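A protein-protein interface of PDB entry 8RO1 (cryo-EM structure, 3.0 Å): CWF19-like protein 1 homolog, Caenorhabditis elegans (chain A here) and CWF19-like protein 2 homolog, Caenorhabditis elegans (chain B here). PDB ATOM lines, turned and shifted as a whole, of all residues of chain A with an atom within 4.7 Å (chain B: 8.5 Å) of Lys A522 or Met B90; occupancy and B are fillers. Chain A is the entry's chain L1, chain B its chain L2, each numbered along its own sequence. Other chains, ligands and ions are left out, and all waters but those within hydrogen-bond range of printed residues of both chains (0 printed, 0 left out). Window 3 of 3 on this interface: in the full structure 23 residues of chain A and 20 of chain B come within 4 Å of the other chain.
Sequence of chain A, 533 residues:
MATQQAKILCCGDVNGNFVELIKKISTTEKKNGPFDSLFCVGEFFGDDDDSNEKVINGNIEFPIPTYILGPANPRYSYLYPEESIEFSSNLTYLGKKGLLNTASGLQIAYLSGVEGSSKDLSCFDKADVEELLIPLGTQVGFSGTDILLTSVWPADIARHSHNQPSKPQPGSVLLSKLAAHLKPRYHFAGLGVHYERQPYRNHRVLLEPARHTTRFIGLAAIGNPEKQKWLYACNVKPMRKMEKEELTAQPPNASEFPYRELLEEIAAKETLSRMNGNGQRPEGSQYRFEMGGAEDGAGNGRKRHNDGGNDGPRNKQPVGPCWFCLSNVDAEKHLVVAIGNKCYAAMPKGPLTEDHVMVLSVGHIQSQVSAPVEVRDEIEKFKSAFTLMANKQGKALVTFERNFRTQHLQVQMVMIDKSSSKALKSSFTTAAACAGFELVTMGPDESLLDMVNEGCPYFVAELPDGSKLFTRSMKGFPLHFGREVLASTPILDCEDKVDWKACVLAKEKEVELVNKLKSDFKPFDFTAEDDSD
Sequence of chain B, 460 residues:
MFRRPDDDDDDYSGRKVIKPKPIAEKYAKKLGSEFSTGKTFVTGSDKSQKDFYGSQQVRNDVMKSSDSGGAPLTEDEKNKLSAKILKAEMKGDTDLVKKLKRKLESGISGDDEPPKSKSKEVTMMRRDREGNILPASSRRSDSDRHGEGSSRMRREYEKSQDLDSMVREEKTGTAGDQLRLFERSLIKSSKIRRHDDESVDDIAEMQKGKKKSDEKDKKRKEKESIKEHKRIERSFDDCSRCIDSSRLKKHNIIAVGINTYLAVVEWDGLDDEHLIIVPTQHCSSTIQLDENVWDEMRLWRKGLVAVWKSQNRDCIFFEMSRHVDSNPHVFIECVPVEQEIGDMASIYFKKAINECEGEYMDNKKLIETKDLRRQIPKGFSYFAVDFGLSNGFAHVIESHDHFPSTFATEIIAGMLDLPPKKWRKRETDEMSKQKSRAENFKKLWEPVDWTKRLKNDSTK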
ATOM      1  N   VAL A 337     -26.313 -21.167  11.378  1.00  0.00           N
ATOM      2  CA  VAL A 337     -26.963 -20.516  12.514  1.00  0.00           C
ATOM      3  C   VAL A 337     -25.998 -19.623  13.277  1.00  0.00           C
ATOM      4  O   VAL A 337     -26.304 -18.461  13.545  1.00  0.00           O
ATOM      5  CB  VAL A 337     -27.581 -21.589  13.444  1.00  0.00           C
ATOM      6  CG1 VAL A 337     -28.235 -20.955  14.680  1.00  0.00           C
ATOM      7  CG2 VAL A 337     -28.601 -22.456  12.677  1.00  0.00           C
ATOM      8  N   ALA A 338     -24.826 -20.142  13.637  1.00  0.00           N
ATOM      9  CA  ALA A 338     -23.872 -19.378  14.427  1.00  0.00           C
ATOM     10  C   ALA A 338     -22.460 -19.827  14.102  1.00  0.00           C
ATOM     11  O   ALA A 338     -22.237 -20.960  13.680  1.00  0.00           O
ATOM     12  CB  ALA A 338     -24.144 -19.559  15.927  1.00  0.00           C
ATOM     13  N   ILE A 339     -21.520 -18.892  14.222  1.00  0.00           N
ATOM     14  CA  ILE A 339     -20.226 -18.970  13.551  1.00  0.00           C
ATOM     15  C   ILE A 339     -19.211 -18.423  14.549  1.00  0.00           C
ATOM     16  O   ILE A 339     -18.826 -17.251  14.472  1.00  0.00           O
ATOM     17  CB  ILE A 339     -20.198 -18.219  12.195  1.00  0.00           C
ATOM     18  CG1 ILE A 339     -21.303 -18.728  11.255  1.00  0.00           C
ATOM     19  CG2 ILE A 339     -18.866 -18.422  11.471  1.00  0.00           C
ATOM     20  CD1 ILE A 339     -21.301 -18.127   9.835  1.00  0.00           C
ATOM     21  N   LYS A 518     -31.175 -18.116  15.556  1.00  0.00           N
ATOM     22  CA  LYS A 518     -30.236 -17.025  15.805  1.00  0.00           C
ATOM     23  C   LYS A 518     -30.727 -16.104  16.915  1.00  0.00           C
ATOM     24  O   LYS A 518     -29.952 -15.716  17.798  1.00  0.00           O
ATOM     25  CB  LYS A 518     -30.014 -16.228  14.520  1.00  0.00           C
ATOM     26  CG  LYS A 518     -29.040 -16.871  13.558  1.00  0.00           C
ATOM     27  CD  LYS A 518     -29.027 -16.157  12.219  1.00  0.00           C
ATOM     28  CE  LYS A 518     -28.000 -16.762  11.277  1.00  0.00           C
ATOM     29  NZ  LYS A 518     -28.073 -16.168   9.913  1.00  0.00           N
ATOM     30  N   SER A 519     -32.012 -15.745  16.886  1.00  0.00           N
ATOM     31  CA  SER A 519     -32.560 -14.822  17.876  1.00  0.00           C
ATOM     32  C   SER A 519     -32.515 -15.415  19.279  1.00  0.00           C
ATOM     33  O   SER A 519     -32.074 -14.757  20.229  1.00  0.00           O
ATOM     34  CB  SER A 519     -33.995 -14.449  17.500  1.00  0.00           C
ATOM     35  OG  SER A 519     -34.548 -13.552  18.446  1.00  0.00           O
ATOM     36  N   ASP A 520     -32.980 -16.656  19.431  1.00  0.00           N
ATOM     37  CA  ASP A 520     -32.974 -17.294  20.744  1.00  0.00           C
ATOM     38  C   ASP A 520     -31.554 -17.498  21.259  1.00  0.00           C
ATOM     39  O   ASP A 520     -31.311 -17.423  22.469  1.00  0.00           O
ATOM     40  CB  ASP A 520     -33.714 -18.628  20.672  1.00  0.00           C
ATOM     41  CG  ASP A 520     -35.202 -18.463  20.426  1.00  0.00           C
ATOM     42  OD1 ASP A 520     -35.718 -17.333  20.567  1.00  0.00           O
ATOM     43  OD2 ASP A 520     -35.861 -19.469  20.089  1.00  0.00           O
ATOM     44  N   PHE A 521     -30.620 -17.834  20.369  1.00  0.00           N
ATOM     45  CA  PHE A 521     -29.237 -18.041  20.787  1.00  0.00           C
ATOM     46  C   PHE A 521     -28.519 -16.729  21.102  1.00  0.00           C
ATOM     47  O   PHE A 521     -27.559 -16.731  21.884  1.00  0.00           O
ATOM     48  CB  PHE A 521     -28.476 -18.804  19.702  1.00  0.00           C
ATOM     49  CG  PHE A 521     -27.122 -19.289  20.138  1.00  0.00           C
ATOM     50  CD1 PHE A 521     -26.997 -20.308  21.068  1.00  0.00           C
ATOM     51  CD2 PHE A 521     -25.971 -18.723  19.615  1.00  0.00           C
ATOM     52  CE1 PHE A 521     -25.751 -20.752  21.469  1.00  0.00           C
ATOM     53  CE2 PHE A 521     -24.723 -19.164  20.011  1.00  0.00           C
ATOM     54  CZ  PHE A 521     -24.612 -20.179  20.939  1.00  0.00           C
ATOM     55  N   LYS A 522     -28.944 -15.623  20.486  1.00  0.00           N
ATOM     56  CA  LYS A 522     -28.253 -14.337  20.621  1.00  0.00           C
ATOM     57  C   LYS A 522     -28.013 -13.857  22.053  1.00  0.00           C
ATOM     58  O   LYS A 522     -26.905 -13.357  22.317  1.00  0.00           O
ATOM     59  CB  LYS A 522     -28.999 -13.271  19.798  1.00  0.00           C
ATOM     60  CG  LYS A 522     -28.254 -11.950  19.664  1.00  0.00           C
ATOM     61  CD  LYS A 522     -29.001 -10.998  18.751  1.00  0.00           C
ATOM     62  CE  LYS A 522     -28.299  -9.656  18.652  1.00  0.00           C
ATOM     63  NZ  LYS A 522     -29.008  -8.742  17.717  1.00  0.00           N
ATOM     64  N   PRO A 523     -28.955 -13.948  23.005  1.00  0.00           N
ATOM     65  CA  PRO A 523     -28.582 -13.606  24.392  1.00  0.00           C
ATOM     66  C   PRO A 523     -27.527 -14.527  24.978  1.00  0.00           C
ATOM     67  O   PRO A 523     -26.598 -14.052  25.642  1.00  0.00           O
ATOM     68  CB  PRO A 523     -29.909 -13.718  25.159  1.00  0.00           C
ATOM     69  CG  PRO A 523     -30.966 -13.628  24.148  1.00  0.00           C
ATOM     70  CD  PRO A 523     -30.407 -14.168  22.876  1.00  0.00           C
ATOM     71  N   PHE A 524     -27.640 -15.835  24.750  1.00  0.00           N
ATOM     72  CA  PHE A 524     -26.657 -16.765  25.295  1.00  0.00           C
ATOM     73  C   PHE A 524     -25.328 -16.701  24.558  1.00  0.00           C
ATOM     74  O   PHE A 524     -24.316 -17.161  25.102  1.00  0.00           O
ATOM     75  CB  PHE A 524     -27.198 -18.194  25.262  1.00  0.00           C
ATOM     76  CG  PHE A 524     -28.572 -18.326  25.833  1.00  0.00           C
ATOM     77  CD1 PHE A 524     -28.747 -18.396  27.203  1.00  0.00           C
ATOM     78  CD2 PHE A 524     -29.686 -18.360  25.014  1.00  0.00           C
ATOM     79  CE1 PHE A 524     -29.998 -18.513  27.745  1.00  0.00           C
ATOM     80  CE2 PHE A 524     -30.946 -18.467  25.555  1.00  0.00           C
ATOM     81  CZ  PHE A 524     -31.099 -18.548  26.923  1.00  0.00           C
ATOM     82  N   ASP A 525     -25.313 -16.174  23.332  1.00  0.00           N
ATOM     83  CA  ASP A 525     -24.133 -16.219  22.481  1.00  0.00           C
ATOM     84  C   ASP A 525     -23.002 -15.432  23.132  1.00  0.00           C
ATOM     85  O   ASP A 525     -23.000 -14.197  23.103  1.00  0.00           O
ATOM     86  CB  ASP A 525     -24.473 -15.661  21.095  1.00  0.00           C
ATOM     87  CG  ASP A 525     -23.334 -15.802  20.097  1.00  0.00           C
ATOM     88  OD1 ASP A 525     -22.269 -16.357  20.446  1.00  0.00           O
ATOM     89  OD2 ASP A 525     -23.506 -15.351  18.944  1.00  0.00           O
ATOM     90  N   ALA B  83     -14.396 -17.571   9.942  1.00  0.00           N
ATOM     91  CA  ALA B  83     -15.578 -17.688  10.783  1.00  0.00           C
ATOM     92  C   ALA B  83     -15.948 -16.370  11.472  1.00  0.00           C
ATOM     93  O   ALA B  83     -17.131 -16.030  11.572  1.00  0.00           O
ATOM     94  CB  ALA B  83     -15.308 -18.799  11.802  1.00  0.00           C
ATOM     95  N   LYS B  84     -14.955 -15.606  11.923  1.00  0.00           N
ATOM     96  CA  LYS B  84     -15.179 -14.329  12.604  1.00  0.00           C
ATOM     97  C   LYS B  84     -15.943 -13.264  11.803  1.00  0.00           C
ATOM     98  O   LYS B  84     -16.421 -12.300  12.410  1.00  0.00           O
ATOM     99  CB  LYS B  84     -13.839 -13.733  13.045  1.00  0.00           C
ATOM    100  CG  LYS B  84     -13.219 -14.406  14.264  1.00  0.00           C
ATOM    101  CD  LYS B  84     -11.978 -13.666  14.739  1.00  0.00           C
ATOM    102  CE  LYS B  84     -11.387 -14.314  15.980  1.00  0.00           C
ATOM    103  NZ  LYS B  84     -10.248 -13.531  16.532  1.00  0.00           N
ATOM    104  N   ILE B  85     -16.049 -13.384  10.475  1.00  0.00           N
ATOM    105  CA  ILE B  85     -16.779 -12.386   9.677  1.00  0.00           C
ATOM    106  C   ILE B  85     -18.242 -12.222  10.114  1.00  0.00           C
ATOM    107  O   ILE B  85     -18.679 -11.107  10.424  1.00  0.00           O
ATOM    108  CB  ILE B  85     -16.669 -12.749   8.181  1.00  0.00           C
ATOM    109  CG1 ILE B  85     -15.244 -12.471   7.681  1.00  0.00           C
ATOM    110  CG2 ILE B  85     -17.693 -11.969   7.320  1.00  0.00           C
ATOM    111  CD1 ILE B  85     -14.880 -13.189   6.396  1.00  0.00           C
ATOM    112  N   LEU B  86     -19.025 -13.306  10.144  1.00  0.00           N
ATOM    113  CA  LEU B  86     -20.396 -13.203  10.664  1.00  0.00           C
ATOM    114  C   LEU B  86     -20.397 -12.877  12.152  1.00  0.00           C
ATOM    115  O   LEU B  86     -21.312 -12.210  12.651  1.00  0.00           O
ATOM    116  CB  LEU B  86     -21.212 -14.476  10.415  1.00  0.00           C
ATOM    117  CG  LEU B  86     -22.673 -14.481  10.950  1.00  0.00           C
ATOM    118  CD1 LEU B  86     -23.505 -13.421  10.242  1.00  0.00           C
ATOM    119  CD2 LEU B  86     -23.363 -15.810  10.819  1.00  0.00           C
ATOM    120  N   LYS B  87     -19.402 -13.394  12.872  1.00  0.00           N
ATOM    121  CA  LYS B  87     -19.302 -13.220  14.318  1.00  0.00           C
ATOM    122  C   LYS B  87     -19.303 -11.751  14.717  1.00  0.00           C
ATOM    123  O   LYS B  87     -19.940 -11.372  15.708  1.00  0.00           O
ATOM    124  CB  LYS B  87     -18.000 -13.877  14.771  1.00  0.00           C
ATOM    125  CG  LYS B  87     -17.883 -14.391  16.162  1.00  0.00           C
ATOM    126  CD  LYS B  87     -16.443 -14.884  16.317  1.00  0.00           C
ATOM    127  CE  LYS B  87     -16.205 -15.524  17.634  1.00  0.00           C
ATOM    128  NZ  LYS B  87     -16.306 -14.574  18.761  1.00  0.00           N
ATOM    129  N   ALA B  88     -18.615 -10.907  13.955  1.00  0.00           N
ATOM    130  CA  ALA B  88     -18.731  -9.468  14.162  1.00  0.00           C
ATOM    131  C   ALA B  88     -20.115  -8.956  13.777  1.00  0.00           C
ATOM    132  O   ALA B  88     -20.673  -8.085  14.454  1.00  0.00           O
ATOM    133  CB  ALA B  88     -17.655  -8.747  13.361  1.00  0.00           C
ATOM    134  N   GLU B  89     -20.687  -9.490  12.694  1.00  0.00           N
ATOM    135  CA  GLU B  89     -22.024  -9.084  12.268  1.00  0.00           C
ATOM    136  C   GLU B  89     -23.107  -9.521  13.248  1.00  0.00           C
ATOM    137  O   GLU B  89     -24.151  -8.866  13.339  1.00  0.00           O
ATOM    138  CB  GLU B  89     -22.313  -9.651  10.878  1.00  0.00           C
ATOM    139  CG  GLU B  89     -21.488  -9.046   9.754  1.00  0.00           C
ATOM    140  CD  GLU B  89     -21.943  -9.502   8.381  1.00  0.00           C
ATOM    141  OE1 GLU B  89     -22.876 -10.327   8.303  1.00  0.00           O
ATOM    142  OE2 GLU B  89     -21.363  -9.035   7.378  1.00  0.00           O
ATOM    143  N   MET B  90     -22.893 -10.618  13.979  1.00  0.00           N
ATOM    144  CA  MET B  90     -23.809 -10.960  15.065  1.00  0.00           C
ATOM    145  C   MET B  90     -23.828  -9.884  16.140  1.00  0.00           C
ATOM    146  O   MET B  90     -24.876  -9.634  16.748  1.00  0.00           O
ATOM    147  CB  MET B  90     -23.434 -12.305  15.678  1.00  0.00           C
ATOM    148  CG  MET B  90     -23.685 -13.481  14.766  1.00  0.00           C
ATOM    149  SD  MET B  90     -22.655 -14.880  15.205  1.00  0.00           S
ATOM    150  CE  MET B  90     -23.913 -15.999  15.794  1.00  0.00           C
ATOM    151  N   LYS B  91     -22.689  -9.240  16.389  1.00  0.00           N
ATOM    152  CA  LYS B  91     -22.658  -8.122  17.321  1.00  0.00           C
ATOM    153  C   LYS B  91     -23.258  -6.870  16.698  1.00  0.00           C
ATOM    154  O   LYS B  91     -23.837  -6.044  17.410  1.00  0.00           O
ATOM    155  CB  LYS B  91     -21.221  -7.841  17.766  1.00  0.00           C
ATOM    156  CG  LYS B  91     -21.118  -6.953  18.997  1.00  0.00           C
ATOM    157  CD  LYS B  91     -19.672  -6.686  19.384  1.00  0.00           C
ATOM    158  CE  LYS B  91     -19.576  -5.597  20.438  1.00  0.00           C
ATOM    159  NZ  LYS B  91     -18.171  -5.340  20.855  1.00  0.00           N
ATOM    160  N   GLY B  92     -23.130  -6.719  15.381  1.00  0.00           N
ATOM    161  CA  GLY B  92     -23.743  -5.625  14.660  1.00  0.00           C
ATOM    162  C   GLY B  92     -22.953  -4.336  14.661  1.00  0.00           C
ATOM    163  O   GLY B  92     -23.424  -3.345  14.091  1.00  0.00           O
ATOM    164  N   ASP B  93     -21.771  -4.313  15.273  1.00  0.00           N
ATOM    165  CA  ASP B  93     -20.854  -3.185  15.135  1.00  0.00           C
ATOM    166  C   ASP B  93     -20.234  -3.285  13.746  1.00  0.00           C
ATOM    167  O   ASP B  93     -19.352  -4.109  13.501  1.00  0.00           O
ATOM    168  CB  ASP B  93     -19.806  -3.226  16.243  1.00  0.00           C
ATOM    169  CG  ASP B  93     -18.827  -2.052  16.197  1.00  0.00           C
ATOM    170  OD1 ASP B  93     -18.912  -1.195  15.291  1.00  0.00           O
ATOM    171  OD2 ASP B  93     -17.951  -1.993  17.085  1.00  0.00           O
ATOM    172  N   VAL B  97     -16.974  -5.440  11.980  1.00  0.00           N
ATOM    173  CA  VAL B  97     -17.127  -6.296  10.798  1.00  0.00           C
ATOM    174  C   VAL B  97     -15.989  -6.054   9.813  1.00  0.00           C
ATOM    175  O   VAL B  97     -15.381  -6.998   9.294  1.00  0.00           O
ATOM    176  CB  VAL B  97     -18.504  -6.060  10.146  1.00  0.00           C
ATOM    177  CG1 VAL B  97     -18.618  -6.781   8.799  1.00  0.00           C
ATOM    178  CG2 VAL B  97     -19.623  -6.507  11.083  1.00  0.00           C
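Printed residues of chain A within 4 Å of Leu B86: Ile A339. Of the printed residues of chain B, Ile A339 touches Ala B83 (3.0 Å), Leu B86 (3.3 Å) and Lys B87 (3.5 Å). Printed residues of chain B within 4 Å of Asp A525: Met B90 (3.2 Å). Printed residues of chain A within 4 Å of Ala B83: Ile A339 (3.0 Å).
CE of Met B90 touches CB of Ala A338, at 3.6 Å. O of Ala B83 touches CG2 of Ile A339 (3.0 Å). Leu B86 touches Ile A339 (CD2 to CD1, 3.3 Å). Ile A339 touches Lys B87 (O to CG, 3.5 Å). O of Met B90 touches CE of Lys A522 (3.9 Å). CE of Met B90 touches OD2 of Asp A525 (3.2 Å).
Of the 11 printed residues of chain A, 4 touch a printed residue of chain B. Hydrophobic or aromatic side chains of chain B that line the printed part of chain A: Ala B83, Leu B86 and Met B90. Along chain B the printed residues that touch a printed residue of chain A span positions 83 to 90. Among the printed residues, 6 pairs touch across the chains.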
